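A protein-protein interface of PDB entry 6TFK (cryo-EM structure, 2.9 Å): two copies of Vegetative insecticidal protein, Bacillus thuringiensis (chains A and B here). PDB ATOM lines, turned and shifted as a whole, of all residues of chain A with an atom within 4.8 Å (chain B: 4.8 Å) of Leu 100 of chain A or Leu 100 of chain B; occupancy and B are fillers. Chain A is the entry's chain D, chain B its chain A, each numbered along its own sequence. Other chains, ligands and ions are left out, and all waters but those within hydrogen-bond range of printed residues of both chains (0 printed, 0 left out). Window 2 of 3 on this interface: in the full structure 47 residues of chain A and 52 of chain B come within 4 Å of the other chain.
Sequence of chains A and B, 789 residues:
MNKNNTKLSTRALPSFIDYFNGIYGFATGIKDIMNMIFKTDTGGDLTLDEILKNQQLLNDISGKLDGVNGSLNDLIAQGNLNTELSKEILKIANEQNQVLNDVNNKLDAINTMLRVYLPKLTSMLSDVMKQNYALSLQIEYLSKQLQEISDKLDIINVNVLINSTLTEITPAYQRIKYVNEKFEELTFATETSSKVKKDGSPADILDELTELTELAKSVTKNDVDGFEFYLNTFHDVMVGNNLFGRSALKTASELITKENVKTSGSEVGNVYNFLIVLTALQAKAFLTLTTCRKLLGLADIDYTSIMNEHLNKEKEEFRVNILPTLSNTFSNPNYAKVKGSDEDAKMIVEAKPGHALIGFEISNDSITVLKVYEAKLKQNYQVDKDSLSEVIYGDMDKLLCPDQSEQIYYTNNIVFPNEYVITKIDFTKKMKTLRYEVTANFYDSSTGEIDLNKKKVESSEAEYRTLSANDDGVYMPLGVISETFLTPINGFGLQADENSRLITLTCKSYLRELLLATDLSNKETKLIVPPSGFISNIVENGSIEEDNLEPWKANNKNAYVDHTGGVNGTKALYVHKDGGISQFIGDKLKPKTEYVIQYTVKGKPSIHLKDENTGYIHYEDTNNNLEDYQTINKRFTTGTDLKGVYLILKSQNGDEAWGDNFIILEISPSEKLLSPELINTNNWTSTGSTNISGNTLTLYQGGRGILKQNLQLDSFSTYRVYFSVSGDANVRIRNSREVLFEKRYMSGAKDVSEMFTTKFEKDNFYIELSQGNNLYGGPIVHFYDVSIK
OE1 of Gln 96 of chain A sits at hydrogen-bond distance from NE2 of Gln 96 of chain B (2.9 Å).
The side-chain amide nitrogen (NE2) of Gln 96 of chain B sits close to the backbone NH (N) of Asn 97 of chain A (3.3 Å).
Of the 9 printed residues of chain A, 4 touch a printed residue of chain B.
Hydrophobic or aromatic side chains of chain A that line the printed part of chain B: Leu 100.
Among the printed residues, 7 pairs touch across the chains.
Among the printed residues, no Asp or Glu carboxylate lies within 4 Å of a Lys or Arg side-chain nitrogen of the other chain.
Among the printed residues, merely in contact across the chains: Leu 100 of chain A with Leu 100 of chain B (3.3 Å), Asn 104 of chain A with Val 103 of chain B (3.3 Å), Leu 100 of chain A with Gln 96 of chain B (3.5 Å), Asn 104 of chain A with Val 99 of chain B (3.5 Å) and Asn 104 of chain A with Asp 102 of chain B (3.9 Å).
Printed residues of chain B within 4 Å of Gln 96 of chain A: Gln 96 (2.9 Å).
Of the printed residues of chain B, Asn 97 of chain A touches Gln 96.
Leu 100 of chain A touches just these residues of chain B: Gln 96 and Leu 100.
Val 103 of chain A touches none of the printed residues of chain B.
Of the printed residues of chain A, Val 99 of chain B touches Asn 104 (3.5 Å).
Leu 100 of chain B touches just one residue of chain A: Leu 100 (3.3 Å).
Printed residues of chain A within 4 Å of Asp 102 of chain B: Asn 104.
Of the printed residues of chain A, Val 103 of chain B touches Asn 104 (3.3 Å).
The nearest printed residue of chain A that does not touch Val 103 of chain B is Leu 100 of chain A (4.8 Å).
Gln 96 of chain B touches its own counterpart, Gln 96 of chain A.
Asn 97 of chain A touches Gln 96 of chain B, but with the chains exchanged Gln 96 of chain A does not touch Asn 97 of chain B (8.2 Å).
Leu 100 of chain A touches its own counterpart, Leu 100 of chain B.
Asn 104 of chain A touches Asp 102 of chain B, but with the chains exchanged Asp 102 of chain A does not touch Asn 104 of chain B (11.7 Å).
9 positions are printed for both chains.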
ATOM      1  N   GLN A  96     -17.502  35.547  21.270  1.00  0.00           N
ATOM      2  CA  GLN A  96     -17.688  34.515  22.284  1.00  0.00           C
ATOM      3  C   GLN A  96     -17.291  33.146  21.746  1.00  0.00           C
ATOM      4  O   GLN A  96     -16.581  32.382  22.412  1.00  0.00           O
ATOM      5  CB  GLN A  96     -19.142  34.508  22.757  1.00  0.00           C
ATOM      6  CG  GLN A  96     -19.383  33.711  24.027  1.00  0.00           C
ATOM      7  CD  GLN A  96     -20.857  33.585  24.364  1.00  0.00           C
ATOM      8  OE1 GLN A  96     -21.685  33.337  23.489  1.00  0.00           O
ATOM      9  NE2 GLN A  96     -21.191  33.761  25.638  1.00  0.00           N
ATOM     10  N   ASN A  97     -17.733  32.821  20.529  1.00  0.00           N
ATOM     11  CA  ASN A  97     -17.440  31.508  19.966  1.00  0.00           C
ATOM     12  C   ASN A  97     -15.944  31.322  19.746  1.00  0.00           C
ATOM     13  O   ASN A  97     -15.401  30.241  20.006  1.00  0.00           O
ATOM     14  CB  ASN A  97     -18.204  31.322  18.656  1.00  0.00           C
ATOM     15  CG  ASN A  97     -17.953  29.970  18.022  1.00  0.00           C
ATOM     16  OD1 ASN A  97     -18.584  28.977  18.381  1.00  0.00           O
ATOM     17  ND2 ASN A  97     -17.028  29.925  17.072  1.00  0.00           N
ATOM     18  N   GLN A  98     -15.253  32.366  19.283  1.00  0.00           N
ATOM     19  CA  GLN A  98     -13.825  32.226  19.015  1.00  0.00           C
ATOM     20  C   GLN A  98     -13.020  32.152  20.308  1.00  0.00           C
ATOM     21  O   GLN A  98     -12.054  31.385  20.397  1.00  0.00           O
ATOM     22  CB  GLN A  98     -13.334  33.376  18.135  1.00  0.00           C
ATOM     23  CG  GLN A  98     -13.601  34.763  18.689  1.00  0.00           C
ATOM     24  CD  GLN A  98     -13.059  35.862  17.793  1.00  0.00           C
ATOM     25  OE1 GLN A  98     -13.759  36.826  17.481  1.00  0.00           O
ATOM     26  NE2 GLN A  98     -11.805  35.724  17.377  1.00  0.00           N
ATOM     27  N   VAL A  99     -13.397  32.933  21.325  1.00  0.00           N
ATOM     28  CA  VAL A  99     -12.694  32.807  22.599  1.00  0.00           C
ATOM     29  C   VAL A  99     -12.955  31.435  23.210  1.00  0.00           C
ATOM     30  O   VAL A  99     -12.071  30.857  23.857  1.00  0.00           O
ATOM     31  CB  VAL A  99     -13.087  33.945  23.562  1.00  0.00           C
ATOM     32  CG1 VAL A  99     -14.557  33.868  23.933  1.00  0.00           C
ATOM     33  CG2 VAL A  99     -12.215  33.910  24.809  1.00  0.00           C
ATOM     34  N   LEU A 100     -14.149  30.876  22.998  1.00  0.00           N
ATOM     35  CA  LEU A 100     -14.419  29.528  23.486  1.00  0.00           C
ATOM     36  C   LEU A 100     -13.593  28.493  22.733  1.00  0.00           C
ATOM     37  O   LEU A 100     -13.117  27.522  23.328  1.00  0.00           O
ATOM     38  CB  LEU A 100     -15.911  29.221  23.369  1.00  0.00           C
ATOM     39  CG  LEU A 100     -16.793  29.930  24.396  1.00  0.00           C
ATOM     40  CD1 LEU A 100     -18.267  29.717  24.071  1.00  0.00           C
ATOM     41  CD2 LEU A 100     -16.448  29.451  25.803  1.00  0.00           C
ATOM     42  N   ASN A 101     -13.419  28.678  21.424  1.00  0.00           N
ATOM     43  CA  ASN A 101     -12.535  27.798  20.666  1.00  0.00           C
ATOM     44  C   ASN A 101     -11.102  27.887  21.181  1.00  0.00           C
ATOM     45  O   ASN A 101     -10.390  26.876  21.254  1.00  0.00           O
ATOM     46  CB  ASN A 101     -12.593  28.156  19.182  1.00  0.00           C
ATOM     47  CG  ASN A 101     -11.525  27.452  18.369  1.00  0.00           C
ATOM     48  OD1 ASN A 101     -11.112  26.339  18.694  1.00  0.00           O
ATOM     49  ND2 ASN A 101     -11.066  28.103  17.306  1.00  0.00           N
ATOM     50  N   ASP A 102     -10.658  29.096  21.527  1.00  0.00           N
ATOM     51  CA  ASP A 102      -9.325  29.263  22.097  1.00  0.00           C
ATOM     52  C   ASP A 102      -9.200  28.506  23.412  1.00  0.00           C
ATOM     53  O   ASP A 102      -8.210  27.802  23.650  1.00  0.00           O
ATOM     54  CB  ASP A 102      -9.027  30.749  22.299  1.00  0.00           C
ATOM     55  CG  ASP A 102      -7.635  30.996  22.844  1.00  0.00           C
ATOM     56  OD1 ASP A 102      -6.657  30.783  22.097  1.00  0.00           O
ATOM     57  OD2 ASP A 102      -7.519  31.404  24.019  1.00  0.00           O
ATOM     58  N   VAL A 103     -10.191  28.661  24.292  1.00  0.00           N
ATOM     59  CA  VAL A 103     -10.219  27.886  25.533  1.00  0.00           C
ATOM     60  C   VAL A 103     -10.111  26.400  25.217  1.00  0.00           C
ATOM     61  O   VAL A 103      -9.309  25.670  25.815  1.00  0.00           O
ATOM     62  CB  VAL A 103     -11.498  28.197  26.331  1.00  0.00           C
ATOM     63  CG1 VAL A 103     -11.578  27.325  27.577  1.00  0.00           C
ATOM     64  CG2 VAL A 103     -11.548  29.666  26.700  1.00  0.00           C
ATOM     65  N   ASN A 104     -10.934  25.933  24.278  1.00  0.00           N
ATOM     66  CA  ASN A 104     -10.939  24.527  23.899  1.00  0.00           C
ATOM     67  C   ASN A 104      -9.537  24.053  23.546  1.00  0.00           C
ATOM     68  O   ASN A 104      -9.032  23.080  24.116  1.00  0.00           O
ATOM     69  CB  ASN A 104     -11.891  24.317  22.717  1.00  0.00           C
ATOM     70  CG  ASN A 104     -12.055  22.854  22.345  1.00  0.00           C
ATOM     71  OD1 ASN A 104     -11.242  22.008  22.717  1.00  0.00           O
ATOM     72  ND2 ASN A 104     -13.112  22.549  21.601  1.00  0.00           N
ATOM     73  N   GLN B  96     -21.804  26.469  18.569  1.00  0.00           N
ATOM     74  CA  GLN B  96     -21.169  26.905  19.808  1.00  0.00           C
ATOM     75  C   GLN B  96     -21.514  25.964  20.956  1.00  0.00           C
ATOM     76  O   GLN B  96     -20.637  25.551  21.724  1.00  0.00           O
ATOM     77  CB  GLN B  96     -21.598  28.336  20.135  1.00  0.00           C
ATOM     78  CG  GLN B  96     -20.774  28.998  21.226  1.00  0.00           C
ATOM     79  CD  GLN B  96     -21.307  30.365  21.611  1.00  0.00           C
ATOM     80  OE1 GLN B  96     -22.519  30.575  21.675  1.00  0.00           O
ATOM     81  NE2 GLN B  96     -20.404  31.305  21.862  1.00  0.00           N
ATOM     82  N   ASN B  97     -22.793  25.604  21.084  1.00  0.00           N
ATOM     83  CA  ASN B  97     -23.209  24.751  22.191  1.00  0.00           C
ATOM     84  C   ASN B  97     -22.564  23.373  22.099  1.00  0.00           C
ATOM     85  O   ASN B  97     -22.140  22.807  23.114  1.00  0.00           O
ATOM     86  CB  ASN B  97     -24.732  24.632  22.213  1.00  0.00           C
ATOM     87  CG  ASN B  97     -25.233  23.770  23.352  1.00  0.00           C
ATOM     88  OD1 ASN B  97     -25.368  24.235  24.483  1.00  0.00           O
ATOM     89  ND2 ASN B  97     -25.513  22.506  23.059  1.00  0.00           N
ATOM     90  N   GLN B  98     -22.462  22.820  20.888  1.00  0.00           N
ATOM     91  CA  GLN B  98     -21.892  21.483  20.750  1.00  0.00           C
ATOM     92  C   GLN B  98     -20.383  21.496  20.971  1.00  0.00           C
ATOM     93  O   GLN B  98     -19.835  20.570  21.582  1.00  0.00           O
ATOM     94  CB  GLN B  98     -22.235  20.897  19.380  1.00  0.00           C
ATOM     95  CG  GLN B  98     -21.819  21.750  18.197  1.00  0.00           C
ATOM     96  CD  GLN B  98     -22.169  21.108  16.866  1.00  0.00           C
ATOM     97  OE1 GLN B  98     -22.749  21.747  15.989  1.00  0.00           O
ATOM     98  NE2 GLN B  98     -21.813  19.838  16.709  1.00  0.00           N
ATOM     99  N   VAL B  99     -19.688  22.533  20.495  1.00  0.00           N
ATOM    100  CA  VAL B  99     -18.257  22.604  20.779  1.00  0.00           C
ATOM    101  C   VAL B  99     -18.027  22.808  22.272  1.00  0.00           C
ATOM    102  O   VAL B  99     -17.050  22.296  22.833  1.00  0.00           O
ATOM    103  CB  VAL B  99     -17.580  23.706  19.941  1.00  0.00           C
ATOM    104  CG1 VAL B  99     -18.103  25.080  20.311  1.00  0.00           C
ATOM    105  CG2 VAL B  99     -16.068  23.643  20.106  1.00  0.00           C
ATOM    106  N   LEU B 100     -18.926  23.530  22.948  1.00  0.00           N
ATOM    107  CA  LEU B 100     -18.802  23.678  24.395  1.00  0.00           C
ATOM    108  C   LEU B 100     -19.044  22.352  25.106  1.00  0.00           C
ATOM    109  O   LEU B 100     -18.372  22.042  26.094  1.00  0.00           O
ATOM    110  CB  LEU B 100     -19.777  24.742  24.895  1.00  0.00           C
ATOM    111  CG  LEU B 100     -19.432  26.173  24.477  1.00  0.00           C
ATOM    112  CD1 LEU B 100     -20.588  27.109  24.784  1.00  0.00           C
ATOM    113  CD2 LEU B 100     -18.159  26.637  25.164  1.00  0.00           C
ATOM    114  N   ASN B 101     -20.002  21.560  24.621  1.00  0.00           N
ATOM    115  CA  ASN B 101     -20.203  20.223  25.174  1.00  0.00           C
ATOM    116  C   ASN B 101     -18.963  19.357  24.976  1.00  0.00           C
ATOM    117  O   ASN B 101     -18.593  18.569  25.857  1.00  0.00           O
ATOM    118  CB  ASN B 101     -21.422  19.571  24.521  1.00  0.00           C
ATOM    119  CG  ASN B 101     -21.541  18.096  24.850  1.00  0.00           C
ATOM    120  OD1 ASN B 101     -21.142  17.654  25.926  1.00  0.00           O
ATOM    121  ND2 ASN B 101     -22.088  17.326  23.918  1.00  0.00           N
ATOM    122  N   ASP B 102     -18.321  19.478  23.813  1.00  0.00           N
ATOM    123  CA  ASP B 102     -17.083  18.743  23.568  1.00  0.00           C
ATOM    124  C   ASP B 102     -16.005  19.154  24.561  1.00  0.00           C
ATOM    125  O   ASP B 102     -15.314  18.305  25.139  1.00  0.00           O
ATOM    126  CB  ASP B 102     -16.614  18.978  22.132  1.00  0.00           C
ATOM    127  CG  ASP B 102     -15.360  18.197  21.793  1.00  0.00           C
ATOM    128  OD1 ASP B 102     -15.445  16.955  21.686  1.00  0.00           O
ATOM    129  OD2 ASP B 102     -14.291  18.823  21.634  1.00  0.00           O
ATOM    130  N   VAL B 103     -15.831  20.464  24.752  1.00  0.00           N
ATOM    131  CA  VAL B 103     -14.900  20.954  25.767  1.00  0.00           C
ATOM    132  C   VAL B 103     -15.228  20.332  27.118  1.00  0.00           C
ATOM    133  O   VAL B 103     -14.350  19.823  27.824  1.00  0.00           O
ATOM    134  CB  VAL B 103     -14.942  22.492  25.837  1.00  0.00           C
ATOM    135  CG1 VAL B 103     -14.017  23.006  26.931  1.00  0.00           C
ATOM    136  CG2 VAL B 103     -14.571  23.095  24.495  1.00  0.00           C
ATOM    137  N   ASN B 104     -16.506  20.379  27.496  1.00  0.00           N
ATOM    138  CA  ASN B 104     -16.942  19.836  28.776  1.00  0.00           C
ATOM    139  C   ASN B 104     -16.487  18.393  28.938  1.00  0.00           C
ATOM    140  O   ASN B 104     -15.824  18.041  29.920  1.00  0.00           O
ATOM    141  CB  ASN B 104     -18.466  19.940  28.886  1.00  0.00           C
ATOM    142  CG  ASN B 104     -18.995  19.471  30.234  1.00  0.00           C
ATOM    143  OD1 ASN B 104     -18.361  18.675  30.925  1.00  0.00           O
ATOM    144  ND2 ASN B 104     -20.167  19.968  30.610  1.00  0.00           N
